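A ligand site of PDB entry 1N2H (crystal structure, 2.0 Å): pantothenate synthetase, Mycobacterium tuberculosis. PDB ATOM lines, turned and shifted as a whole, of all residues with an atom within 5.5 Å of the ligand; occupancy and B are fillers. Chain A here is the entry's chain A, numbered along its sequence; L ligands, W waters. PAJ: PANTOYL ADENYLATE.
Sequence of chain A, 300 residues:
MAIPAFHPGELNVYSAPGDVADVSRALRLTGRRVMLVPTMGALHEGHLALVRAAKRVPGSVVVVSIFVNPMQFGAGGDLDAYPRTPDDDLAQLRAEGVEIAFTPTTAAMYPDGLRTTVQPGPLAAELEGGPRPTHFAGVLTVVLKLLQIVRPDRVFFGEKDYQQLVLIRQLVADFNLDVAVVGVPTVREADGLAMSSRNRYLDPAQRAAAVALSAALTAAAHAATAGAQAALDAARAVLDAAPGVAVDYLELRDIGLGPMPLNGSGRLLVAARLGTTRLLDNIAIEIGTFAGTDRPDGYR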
ATOM      1  N   PRO A  38      -4.685   9.615  11.725  1.00  0.00           N
ATOM      2  CA  PRO A  38      -4.327   9.076  10.404  1.00  0.00           C
ATOM      3  C   PRO A  38      -2.906   9.410  10.028  1.00  0.00           C
ATOM      4  O   PRO A  38      -2.482  10.574  10.170  1.00  0.00           O
ATOM      5  CB  PRO A  38      -5.322   9.764   9.449  1.00  0.00           C
ATOM      6  CG  PRO A  38      -6.532  10.127  10.388  1.00  0.00           C
ATOM      7  CD  PRO A  38      -5.768  10.631  11.627  1.00  0.00           C
ATOM      8  N   THR A  39      -2.152   8.404   9.563  1.00  0.00           N
ATOM      9  CA  THR A  39      -0.767   8.613   9.088  1.00  0.00           C
ATOM     10  C   THR A  39      -0.464   7.668   7.913  1.00  0.00           C
ATOM     11  O   THR A  39      -1.191   6.720   7.652  1.00  0.00           O
ATOM     12  CB  THR A  39       0.317   8.289  10.169  1.00  0.00           C
ATOM     13  OG1 THR A  39       0.569   6.869  10.193  1.00  0.00           O
ATOM     14  CG2 THR A  39      -0.137   8.746  11.556  1.00  0.00           C
ATOM     15  N   MET A  40       0.622   7.963   7.201  1.00  0.00           N
ATOM     16  CA  MET A  40       1.086   7.109   6.138  1.00  0.00           C
ATOM     17  C   MET A  40       2.410   6.445   6.599  1.00  0.00           C
ATOM     18  O   MET A  40       3.266   6.115   5.765  1.00  0.00           O
ATOM     19  CB  MET A  40       1.321   7.897   4.850  1.00  0.00           C
ATOM     20  CG  MET A  40       0.040   8.635   4.369  1.00  0.00           C
ATOM     21  SD  MET A  40      -0.092   8.777   2.574  1.00  0.00           S
ATOM     22  CE  MET A  40       1.178   9.898   2.236  1.00  0.00           C
ATOM     23  N   GLY A  41       2.586   6.278   7.893  1.00  0.00           N
ATOM     24  CA  GLY A  41       3.829   5.647   8.388  1.00  0.00           C
ATOM     25  C   GLY A  41       5.107   6.486   8.377  1.00  0.00           C
ATOM     26  O   GLY A  41       5.054   7.735   8.236  1.00  0.00           O
ATOM     27  N   HIS A  44       7.668  10.072  12.900  1.00  0.00           N
ATOM     28  CA  HIS A  44       8.706  10.884  13.550  1.00  0.00           C
ATOM     29  C   HIS A  44       8.004  11.719  14.633  1.00  0.00           C
ATOM     30  O   HIS A  44       6.793  11.566  14.857  1.00  0.00           O
ATOM     31  CB  HIS A  44       9.429  11.778  12.523  1.00  0.00           C
ATOM     32  CG  HIS A  44       8.495  12.656  11.732  1.00  0.00           C
ATOM     33  ND1 HIS A  44       7.672  13.584  12.322  1.00  0.00           N
ATOM     34  CD2 HIS A  44       8.258  12.731  10.403  1.00  0.00           C
ATOM     35  CE1 HIS A  44       6.940  14.182  11.387  1.00  0.00           C
ATOM     36  NE2 HIS A  44       7.284  13.674  10.212  1.00  0.00           N
ATOM     37  N   GLY A  46       6.809  14.629  14.771  1.00  0.00           N
ATOM     38  CA  GLY A  46       5.650  15.392  14.373  1.00  0.00           C
ATOM     39  C   GLY A  46       4.407  14.518  14.569  1.00  0.00           C
ATOM     40  O   GLY A  46       3.407  14.931  15.170  1.00  0.00           O
ATOM     41  N   HIS A  47       4.463  13.300  14.060  1.00  0.00           N
ATOM     42  CA  HIS A  47       3.358  12.371  14.188  1.00  0.00           C
ATOM     43  C   HIS A  47       3.083  12.068  15.662  1.00  0.00           C
ATOM     44  O   HIS A  47       1.911  11.986  16.078  1.00  0.00           O
ATOM     45  CB  HIS A  47       3.675  11.056  13.469  1.00  0.00           C
ATOM     46  CG  HIS A  47       4.039  11.214  12.025  1.00  0.00           C
ATOM     47  ND1 HIS A  47       5.301  10.976  11.538  1.00  0.00           N
ATOM     48  CD2 HIS A  47       3.272  11.517  10.940  1.00  0.00           C
ATOM     49  CE1 HIS A  47       5.308  11.099  10.224  1.00  0.00           C
ATOM     50  NE2 HIS A  47       4.089  11.430   9.837  1.00  0.00           N
ATOM     51  N   ALA A  49       3.350  13.933  18.263  1.00  0.00           N
ATOM     52  CA  ALA A  49       2.650  15.002  18.969  1.00  0.00           C
ATOM     53  C   ALA A  49       1.151  14.774  18.773  1.00  0.00           C
ATOM     54  O   ALA A  49       0.350  15.063  19.668  1.00  0.00           O
ATOM     55  CB  ALA A  49       3.049  16.392  18.421  1.00  0.00           C
ATOM     56  N   LEU A  50       0.750  14.270  17.605  1.00  0.00           N
ATOM     57  CA  LEU A  50      -0.657  13.975  17.367  1.00  0.00           C
ATOM     58  C   LEU A  50      -1.056  12.820  18.281  1.00  0.00           C
ATOM     59  O   LEU A  50      -2.120  12.846  18.922  1.00  0.00           O
ATOM     60  CB  LEU A  50      -0.899  13.572  15.894  1.00  0.00           C
ATOM     61  CG  LEU A  50      -1.203  14.753  14.933  1.00  0.00           C
ATOM     62  CD1 LEU A  50      -0.001  15.660  14.800  1.00  0.00           C
ATOM     63  CD2 LEU A  50      -1.619  14.215  13.559  1.00  0.00           C
ATOM     64  N   PHE A  67      -1.179   3.754   6.486  1.00  0.00           N
ATOM     65  CA  PHE A  67      -1.604   3.320   5.173  1.00  0.00           C
ATOM     66  C   PHE A  67      -1.075   4.320   4.180  1.00  0.00           C
ATOM     67  O   PHE A  67      -1.469   5.505   4.201  1.00  0.00           O
ATOM     68  CB  PHE A  67      -3.135   3.265   5.095  1.00  0.00           C
ATOM     69  CG  PHE A  67      -3.681   2.839   3.755  1.00  0.00           C
ATOM     70  CD1 PHE A  67      -3.235   1.657   3.154  1.00  0.00           C
ATOM     71  CD2 PHE A  67      -4.603   3.640   3.075  1.00  0.00           C
ATOM     72  CE1 PHE A  67      -3.700   1.274   1.882  1.00  0.00           C
ATOM     73  CE2 PHE A  67      -5.084   3.276   1.818  1.00  0.00           C
ATOM     74  CZ  PHE A  67      -4.627   2.087   1.213  1.00  0.00           C
ATOM     75  N   ASN A  69      -1.604   5.729   1.242  1.00  0.00           N
ATOM     76  CA  ASN A  69      -2.732   5.838   0.320  1.00  0.00           C
ATOM     77  C   ASN A  69      -2.378   6.054  -1.159  1.00  0.00           C
ATOM     78  O   ASN A  69      -2.002   7.147  -1.570  1.00  0.00           O
ATOM     79  CB  ASN A  69      -3.657   6.966   0.853  1.00  0.00           C
ATOM     80  CG  ASN A  69      -4.810   7.212  -0.066  1.00  0.00           C
ATOM     81  OD1 ASN A  69      -5.298   6.273  -0.688  1.00  0.00           O
ATOM     82  ND2 ASN A  69      -5.274   8.470  -0.162  1.00  0.00           N
ATOM     83  N   GLN A  72      -3.688   9.340  -3.322  1.00  0.00           N
ATOM     84  CA  GLN A  72      -3.263  10.720  -3.219  1.00  0.00           C
ATOM     85  C   GLN A  72      -1.914  10.945  -3.895  1.00  0.00           C
ATOM     86  O   GLN A  72      -1.356  12.051  -3.851  1.00  0.00           O
ATOM     87  CB  GLN A  72      -3.238  11.190  -1.773  1.00  0.00           C
ATOM     88  CG  GLN A  72      -2.136  10.583  -0.875  1.00  0.00           C
ATOM     89  CD  GLN A  72      -2.471  10.812   0.602  1.00  0.00           C
ATOM     90  OE1 GLN A  72      -3.479  10.288   1.096  1.00  0.00           O
ATOM     91  NE2 GLN A  72      -1.665  11.621   1.304  1.00  0.00           N
ATOM     92  N   TYR A  82       7.889   6.571  -1.612  1.00  0.00           N
ATOM     93  CA  TYR A  82       7.499   7.007  -0.269  1.00  0.00           C
ATOM     94  C   TYR A  82       8.234   6.191   0.797  1.00  0.00           C
ATOM     95  O   TYR A  82       8.304   4.984   0.706  1.00  0.00           O
ATOM     96  CB  TYR A  82       5.989   6.870  -0.055  1.00  0.00           C
ATOM     97  CG  TYR A  82       5.525   7.775   1.043  1.00  0.00           C
ATOM     98  CD1 TYR A  82       5.420   9.162   0.822  1.00  0.00           C
ATOM     99  CD2 TYR A  82       5.276   7.269   2.327  1.00  0.00           C
ATOM    100  CE1 TYR A  82       5.094  10.026   1.891  1.00  0.00           C
ATOM    101  CE2 TYR A  82       4.939   8.116   3.372  1.00  0.00           C
ATOM    102  CZ  TYR A  82       4.856   9.494   3.154  1.00  0.00           C
ATOM    103  OH  TYR A  82       4.606  10.339   4.201  1.00  0.00           O
ATOM    104  N   VAL A 139      -6.851  12.267  -0.700  1.00  0.00           N
ATOM    105  CA  VAL A 139      -6.771  12.442   0.741  1.00  0.00           C
ATOM    106  C   VAL A 139      -8.196  12.369   1.384  1.00  0.00           C
ATOM    107  O   VAL A 139      -8.427  11.604   2.311  1.00  0.00           O
ATOM    108  CB  VAL A 139      -6.131  13.826   1.107  1.00  0.00           C
ATOM    109  CG1 VAL A 139      -6.292  14.088   2.582  1.00  0.00           C
ATOM    110  CG2 VAL A 139      -4.602  13.872   0.677  1.00  0.00           C
ATOM    111  N   VAL A 142      -9.776   8.819   1.284  1.00  0.00           N
ATOM    112  CA  VAL A 142      -9.293   7.841   2.248  1.00  0.00           C
ATOM    113  C   VAL A 142      -9.656   8.266   3.685  1.00  0.00           C
ATOM    114  O   VAL A 142      -9.981   7.412   4.514  1.00  0.00           O
ATOM    115  CB  VAL A 142      -7.749   7.611   2.113  1.00  0.00           C
ATOM    116  CG1 VAL A 142      -6.976   8.679   2.895  1.00  0.00           C
ATOM    117  CG2 VAL A 142      -7.374   6.187   2.659  1.00  0.00           C
ATOM    118  N   VAL A 143      -9.624   9.565   3.970  1.00  0.00           N
ATOM    119  CA  VAL A 143      -9.934   9.982   5.320  1.00  0.00           C
ATOM    120  C   VAL A 143     -11.409   9.717   5.604  1.00  0.00           C
ATOM    121  O   VAL A 143     -11.745   9.269   6.693  1.00  0.00           O
ATOM    122  CB  VAL A 143      -9.590  11.474   5.606  1.00  0.00           C
ATOM    123  CG1 VAL A 143     -10.262  11.953   6.946  1.00  0.00           C
ATOM    124  CG2 VAL A 143      -8.068  11.628   5.694  1.00  0.00           C
ATOM    125  N   LEU A 146     -11.619   6.055   6.406  1.00  0.00           N
ATOM    126  CA  LEU A 146     -11.029   5.802   7.720  1.00  0.00           C
ATOM    127  C   LEU A 146     -11.986   6.251   8.826  1.00  0.00           C
ATOM    128  O   LEU A 146     -12.137   5.561   9.839  1.00  0.00           O
ATOM    129  CB  LEU A 146      -9.694   6.514   7.845  1.00  0.00           C
ATOM    130  CG  LEU A 146      -8.552   5.888   7.052  1.00  0.00           C
ATOM    131  CD1 LEU A 146      -7.374   6.879   7.054  1.00  0.00           C
ATOM    132  CD2 LEU A 146      -8.101   4.548   7.681  1.00  0.00           C
ATOM    133  N   PHE A 156      -7.217  13.541  14.618  1.00  0.00           N
ATOM    134  CA  PHE A 156      -6.157  14.547  14.748  1.00  0.00           C
ATOM    135  C   PHE A 156      -5.368  14.749  13.481  1.00  0.00           C
ATOM    136  O   PHE A 156      -5.001  13.777  12.804  1.00  0.00           O
ATOM    137  CB  PHE A 156      -5.198  14.157  15.889  1.00  0.00           C
ATOM    138  CG  PHE A 156      -5.875  14.056  17.219  1.00  0.00           C
ATOM    139  CD1 PHE A 156      -6.816  13.043  17.468  1.00  0.00           C
ATOM    140  CD2 PHE A 156      -5.675  15.042  18.174  1.00  0.00           C
ATOM    141  CE1 PHE A 156      -7.568  13.041  18.656  1.00  0.00           C
ATOM    142  CE2 PHE A 156      -6.432  15.058  19.385  1.00  0.00           C
ATOM    143  CZ  PHE A 156      -7.373  14.063  19.613  1.00  0.00           C
ATOM    144  N   PHE A 157      -5.105  16.014  13.164  1.00  0.00           N
ATOM    145  CA  PHE A 157      -4.343  16.387  11.994  1.00  0.00           C
ATOM    146  C   PHE A 157      -3.342  17.484  12.383  1.00  0.00           C
ATOM    147  O   PHE A 157      -3.613  18.317  13.261  1.00  0.00           O
ATOM    148  CB  PHE A 157      -5.281  16.910  10.902  1.00  0.00           C
ATOM    149  CG  PHE A 157      -6.032  15.825  10.172  1.00  0.00           C
ATOM    150  CD1 PHE A 157      -7.327  15.480  10.554  1.00  0.00           C
ATOM    151  CD2 PHE A 157      -5.441  15.134   9.104  1.00  0.00           C
ATOM    152  CE1 PHE A 157      -8.030  14.472   9.910  1.00  0.00           C
ATOM    153  CE2 PHE A 157      -6.145  14.107   8.444  1.00  0.00           C
ATOM    154  CZ  PHE A 157      -7.440  13.771   8.853  1.00  0.00           C
ATOM    155  N   GLY A 158      -2.185  17.480  11.727  1.00  0.00           N
ATOM    156  CA  GLY A 158      -1.180  18.476  12.041  1.00  0.00           C
ATOM    157  C   GLY A 158      -1.363  19.790  11.282  1.00  0.00           C
ATOM    158  O   GLY A 158      -1.854  19.812  10.157  1.00  0.00           O
ATOM    159  N   GLU A 159      -0.997  20.902  11.915  1.00  0.00           N
ATOM    160  CA  GLU A 159      -1.084  22.185  11.236  1.00  0.00           C
ATOM    161  C   GLU A 159       0.003  22.249  10.134  1.00  0.00           C
ATOM    162  O   GLU A 159      -0.023  23.134   9.260  1.00  0.00           O
ATOM    163  CB  GLU A 159      -0.876  23.312  12.246  1.00  0.00           C
ATOM    164  CG  GLU A 159      -2.084  23.524  13.149  1.00  0.00           C
ATOM    165  CD  GLU A 159      -1.933  24.755  14.031  1.00  0.00           C
ATOM    166  OE1 GLU A 159      -0.955  25.493  13.866  1.00  0.00           O
ATOM    167  OE2 GLU A 159      -2.810  24.989  14.885  1.00  0.00           O
ATOM    168  N   LYS A 160       0.963  21.337  10.193  1.00  0.00           N
ATOM    169  CA  LYS A 160       2.021  21.276   9.188  1.00  0.00           C
ATOM    170  C   LYS A 160       1.429  21.192   7.793  1.00  0.00           C
ATOM    171  O   LYS A 160       1.906  21.822   6.865  1.00  0.00           O
ATOM    172  CB  LYS A 160       2.941  20.062   9.370  1.00  0.00           C
ATOM    173  CG  LYS A 160       3.881  19.961   8.169  1.00  0.00           C
ATOM    174  CD  LYS A 160       5.156  19.311   8.482  1.00  0.00           C
ATOM    175  CE  LYS A 160       6.206  19.773   7.493  1.00  0.00           C
ATOM    176  NZ  LYS A 160       5.723  20.069   6.127  1.00  0.00           N
ATOM    177  N   ASP A 161       0.403  20.363   7.629  1.00  0.00           N
ATOM    178  CA  ASP A 161      -0.266  20.276   6.339  1.00  0.00           C
ATOM    179  C   ASP A 161      -1.577  21.046   6.561  1.00  0.00           C
ATOM    180  O   ASP A 161      -2.676  20.466   6.623  1.00  0.00           O
ATOM    181  CB  ASP A 161      -0.522  18.818   6.011  1.00  0.00           C
ATOM    182  CG  ASP A 161       0.764  18.044   5.896  1.00  0.00           C
ATOM    183  OD1 ASP A 161       1.442  18.216   4.894  1.00  0.00           O
ATOM    184  OD2 ASP A 161       1.110  17.305   6.834  1.00  0.00           O
ATOM    185  N   GLN A 164      -4.454  20.652   4.021  1.00  0.00           N
ATOM    186  CA  GLN A 164      -5.108  19.389   4.221  1.00  0.00           C
ATOM    187  C   GLN A 164      -6.066  19.477   5.419  1.00  0.00           C
ATOM    188  O   GLN A 164      -7.187  19.009   5.344  1.00  0.00           O
ATOM    189  CB  GLN A 164      -4.077  18.281   4.479  1.00  0.00           C
ATOM    190  CG  GLN A 164      -4.680  17.050   5.087  1.00  0.00           C
ATOM    191  CD  GLN A 164      -3.663  15.936   5.182  1.00  0.00           C
ATOM    192  OE1 GLN A 164      -3.529  15.130   4.256  1.00  0.00           O
ATOM    193  NE2 GLN A 164      -2.923  15.903   6.291  1.00  0.00           N
ATOM    194  N   VAL A 184      -3.297  20.013  15.480  1.00  0.00           N
ATOM    195  CA  VAL A 184      -2.137  19.979  16.375  1.00  0.00           C
ATOM    196  C   VAL A 184      -1.020  20.845  15.805  1.00  0.00           C
ATOM    197  O   VAL A 184      -0.664  20.735  14.616  1.00  0.00           O
ATOM    198  CB  VAL A 184      -1.651  18.529  16.533  1.00  0.00           C
ATOM    199  CG1 VAL A 184      -0.442  18.453  17.459  1.00  0.00           C
ATOM    200  CG2 VAL A 184      -2.779  17.693  17.100  1.00  0.00           C
ATOM    201  N   PRO A 185      -0.445  21.743  16.638  1.00  0.00           N
ATOM    202  CA  PRO A 185       0.630  22.614  16.163  1.00  0.00           C
ATOM    203  C   PRO A 185       1.821  21.857  15.612  1.00  0.00           C
ATOM    204  O   PRO A 185       2.120  20.711  16.019  1.00  0.00           O
ATOM    205  CB  PRO A 185       1.010  23.436  17.404  1.00  0.00           C
ATOM    206  CG  PRO A 185      -0.241  23.357  18.291  1.00  0.00           C
ATOM    207  CD  PRO A 185      -0.688  21.925  18.088  1.00  0.00           C
ATOM    208  N   THR A 186       2.484  22.522  14.666  1.00  0.00           N
ATOM    209  CA  THR A 186       3.642  21.966  13.998  1.00  0.00           C
ATOM    210  C   THR A 186       4.859  21.725  14.878  1.00  0.00           C
ATOM    211  O   THR A 186       5.334  22.620  15.546  1.00  0.00           O
ATOM    212  CB  THR A 186       4.040  22.887  12.830  1.00  0.00           C
ATOM    213  OG1 THR A 186       2.978  22.850  11.871  1.00  0.00           O
ATOM    214  CG2 THR A 186       5.328  22.426  12.174  1.00  0.00           C
ATOM    215  N   VAL A 187       5.361  20.501  14.857  1.00  0.00           N
ATOM    216  CA  VAL A 187       6.549  20.160  15.622  1.00  0.00           C
ATOM    217  C   VAL A 187       7.716  20.527  14.743  1.00  0.00           C
ATOM    218  O   VAL A 187       7.724  20.183  13.544  1.00  0.00           O
ATOM    219  CB  VAL A 187       6.608  18.654  15.953  1.00  0.00           C
ATOM    220  CG1 VAL A 187       7.931  18.343  16.649  1.00  0.00           C
ATOM    221  CG2 VAL A 187       5.457  18.250  16.876  1.00  0.00           C
ATOM    222  N   ARG A 188       8.694  21.208  15.327  1.00  0.00           N
ATOM    223  CA  ARG A 188       9.895  21.687  14.618  1.00  0.00           C
ATOM    224  C   ARG A 188      11.222  21.238  15.206  1.00  0.00           C
ATOM    225  O   ARG A 188      11.317  20.962  16.395  1.00  0.00           O
ATOM    226  CB  ARG A 188       9.882  23.210  14.627  1.00  0.00           C
ATOM    227  CG  ARG A 188       8.647  23.799  13.968  1.00  0.00           C
ATOM    228  CD  ARG A 188       8.537  25.307  14.191  1.00  0.00           C
ATOM    229  NE  ARG A 188       7.363  25.786  13.497  1.00  0.00           N
ATOM    230  CZ  ARG A 188       7.322  26.059  12.196  1.00  0.00           C
ATOM    231  NH1 ARG A 188       8.414  25.937  11.447  1.00  0.00           N
ATOM    232  NH2 ARG A 188       6.159  26.359  11.619  1.00  0.00           N
ATOM    233  N   ALA A 194      10.469  22.567  10.115  1.00  0.00           N
ATOM    234  CA  ALA A 194       9.273  21.780  10.424  1.00  0.00           C
ATOM    235  C   ALA A 194       9.610  20.312  10.225  1.00  0.00           C
ATOM    236  O   ALA A 194      10.197  19.943   9.207  1.00  0.00           O
ATOM    237  CB  ALA A 194       8.119  22.192   9.506  1.00  0.00           C
ATOM    238  N   MET A 195       9.253  19.458  11.182  1.00  0.00           N
ATOM    239  CA  MET A 195       9.556  18.033  10.991  1.00  0.00           C
ATOM    240  C   MET A 195       8.711  17.406   9.885  1.00  0.00           C
ATOM    241  O   MET A 195       7.502  17.647   9.757  1.00  0.00           O
ATOM    242  CB  MET A 195       9.392  17.257  12.283  1.00  0.00           C
ATOM    243  CG  MET A 195      10.534  17.482  13.257  1.00  0.00           C
ATOM    244  SD  MET A 195      10.415  16.322  14.597  1.00  0.00           S
ATOM    245  CE  MET A 195      11.453  17.149  15.881  1.00  0.00           C
ATOM    246  N   SER A 196       9.375  16.608   9.082  1.00  0.00           N
ATOM    247  CA  SER A 196       8.777  15.943   7.954  1.00  0.00           C
ATOM    248  C   SER A 196       9.557  14.697   7.583  1.00  0.00           C
ATOM    249  O   SER A 196      10.782  14.635   7.753  1.00  0.00           O
ATOM    250  CB  SER A 196       8.777  16.893   6.757  1.00  0.00           C
ATOM    251  OG  SER A 196       8.492  16.182   5.567  1.00  0.00           O
ATOM    252  N   SER A 197       8.846  13.716   7.064  1.00  0.00           N
ATOM    253  CA  SER A 197       9.477  12.484   6.634  1.00  0.00           C
ATOM    254  C   SER A 197      10.378  12.820   5.448  1.00  0.00           C
ATOM    255  O   SER A 197      11.298  12.076   5.138  1.00  0.00           O
ATOM    256  CB  SER A 197       8.397  11.437   6.256  1.00  0.00           C
ATOM    257  OG  SER A 197       7.443  11.960   5.330  1.00  0.00           O
HETATM  258  P   PAJ L   1       1.398  11.885   7.033  1.00  0.00           P
HETATM  259  O1P PAJ L   1       2.241  12.592   6.103  1.00  0.00           O
HETATM  260  O2P PAJ L   1       1.875  10.586   7.586  1.00  0.00           O
HETATM  261  O5' PAJ L   1       1.104  12.947   8.234  1.00  0.00           O
HETATM  262  C5' PAJ L   1       0.230  12.403   8.976  1.00  0.00           C
HETATM  263  C4' PAJ L   1      -0.259  13.512   9.911  1.00  0.00           C
HETATM  264  O4' PAJ L   1       0.847  13.988  10.735  1.00  0.00           O
HETATM  265  C3' PAJ L   1      -0.815  14.757   9.188  1.00  0.00           C
HETATM  266  O3' PAJ L   1      -1.989  15.161   9.857  1.00  0.00           O
HETATM  267  C2' PAJ L   1       0.263  15.757   9.305  1.00  0.00           C
HETATM  268  O2' PAJ L   1      -0.132  17.137   9.166  1.00  0.00           O
HETATM  269  C1' PAJ L   1       0.879  15.419  10.650  1.00  0.00           C
HETATM  270  N9  PAJ L   1       2.210  15.936  10.702  1.00  0.00           N
HETATM  271  C8  PAJ L   1       3.295  15.715   9.906  1.00  0.00           C
HETATM  272  N7  PAJ L   1       4.399  16.343  10.209  1.00  0.00           N
HETATM  273  C5  PAJ L   1       4.039  17.067  11.306  1.00  0.00           C
HETATM  274  C6  PAJ L   1       4.759  17.967  12.147  1.00  0.00           C
HETATM  275  N6  PAJ L   1       6.037  18.275  11.936  1.00  0.00           N
HETATM  276  N1  PAJ L   1       4.073  18.553  13.214  1.00  0.00           N
HETATM  277  C2  PAJ L   1       2.736  18.260  13.472  1.00  0.00           C
HETATM  278  N3  PAJ L   1       1.946  17.391  12.709  1.00  0.00           N
HETATM  279  C4  PAJ L   1       2.679  16.825  11.643  1.00  0.00           C
HETATM  280  O11 PAJ L   1      -1.216  13.608   5.945  1.00  0.00           O
HETATM  281  C11 PAJ L   1      -1.125  12.333   5.630  1.00  0.00           C
HETATM  282  O12 PAJ L   1       0.081  11.552   6.275  1.00  0.00           O
HETATM  283  C12 PAJ L   1      -2.146  11.718   4.683  1.00  0.00           C
HETATM  284  O13 PAJ L   1      -2.594  12.774   3.759  1.00  0.00           O
HETATM  285  C13 PAJ L   1      -3.383  11.076   5.465  1.00  0.00           C
HETATM  286  C14 PAJ L   1      -2.910   9.986   6.492  1.00  0.00           C
HETATM  287  C15 PAJ L   1      -4.231  12.211   6.184  1.00  0.00           C
HETATM  288  C16 PAJ L   1      -4.275  10.439   4.385  1.00  0.00           C
HETATM  289  O14 PAJ L   1      -3.573   9.439   3.654  1.00  0.00           O
HETATM  290  O   HOH W   1      -3.513  12.877  10.497  1.00  0.00           O
HETATM  291  O   HOH W   2       2.963  15.439   6.515  1.00  0.00           O
HETATM  292  O   HOH W   3       4.518   9.778   6.836  1.00  0.00           O
HETATM  293  O   HOH W   4      -3.129  18.105   8.210  1.00  0.00           O
HETATM  294  O   HOH W   5      -3.879   6.867   4.522  1.00  0.00           O
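The backbone carbonyl oxygen (O) of Met 195 lies within hydrogen-bond range of a nitrogen (N6) of the ligand, 2.7 Å away.
N6 of the ligand sits at hydrogen-bond distance from O of Val 187, 3.0 Å away.
The side-chain carboxylate of Asp 161 lies within hydrogen-bond range of an oxygen (O2') of the ligand (2.6 Å).
SD of Met 40 is in hydrogen-bond range of O14 of the ligand (3.7 Å).
An oxygen (O14) of the ligand is in hydrogen-bond range of the side-chain amide oxygen of Gln 72 (2.7 Å).
The backbone NH of Gly 158 is in hydrogen-bond range of an oxygen (O3') of the ligand, 3.0 Å away.
A ring nitrogen (NE2) of His 47 lies within hydrogen-bond range of an oxygen (O2P) of the ligand, at 3.3 Å.
A nitrogen (N1) of the ligand lies within hydrogen-bond range of the backbone NH (N) of Val 187 (2.9 Å).
The side-chain amide oxygen of Gln 164 is in hydrogen-bond range of an oxygen (O13) of the ligand (2.6 Å).
An oxygen (O2') of the ligand sits at hydrogen-bond distance from the backbone carbonyl oxygen (O) of Gly 158 (3.3 Å).
N of Met 40 sits at hydrogen-bond distance from O2P of the ligand, 2.9 Å away.
N of Val 184 lies within hydrogen-bond range of O of Phe 157 (2.8 Å).
N of Phe 67 lies within hydrogen-bond range of O of Thr 39, at 3.2 Å.
The backbone NH (N) of Lys 160 is in hydrogen-bond range of the side-chain hydroxyl (OG1) of Thr 186 (3.0 Å).
N of Gly 46 is in hydrogen-bond range of ND1 of His 44 (2.8 Å).
The side-chain amide oxygen of Gln 72 sits at hydrogen-bond distance from the side-chain amide nitrogen of Asn 69 (2.8 Å).
N of Met 195 sits at hydrogen-bond distance from O of Val 187.
A ring nitrogen (ND1) of His 47 lies within hydrogen-bond range of the backbone NH (N) of His 44 (2.9 Å).
The side-chain hydroxyl (OH) of Tyr 82 sits at hydrogen-bond distance from the side-chain hydroxyl (OG) of Ser 197 (3.5 Å).
Residues that only touch the ligand: Leu 50, Phe 157, Pro 38, Lys 160, Gly 46, Thr 186, Thr 39, His 44, Val 142, Pro 185, Asn 69, Tyr 82, Val 139 and Val 143.
Hydrophobic or aromatic side chains that line the ligand: Pro 38, Met 40, His 44, His 47, Leu 50, Val 139, Val 142, Val 143, Phe 157, Val 187 and Met 195.
Of the 33 residues printed, 22 come within 4 Å of the ligand.
The nearest printed residue that does not touch the ligand is Gly 41 (4.3 Å).
Water W5 lies within hydrogen-bond range of O14 of the ligand (2.7 Å) and O of Phe 67 (2.8 Å).
Water W1 lies within hydrogen-bond range of the backbone carbonyl oxygen of Pro 38 (2.5 Å), an oxygen (O3') of the ligand (2.8 Å) and the backbone carbonyl oxygen of Phe 156 (2.9 Å).
Water W3 lies within hydrogen-bond range of the backbone carbonyl oxygen (O) of Gly 41 (2.5 Å), the side-chain hydroxyl (OH) of Tyr 82 (2.7 Å), an oxygen (O2P) of the ligand (2.9 Å) and a ring nitrogen (NE2) of His 47 (3.5 Å).
Water W2 bridges the side-chain carboxylate of Asp 161 (2.6 Å) and an oxygen (O1P) of the ligand (3.0 Å).
Water W4 lies within hydrogen-bond range of O of Asp 161 (2.9 Å), O of Gly 158 (2.9 Å), NE2 of Gln 164 (2.9 Å) and O2' of the ligand (3.3 Å).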
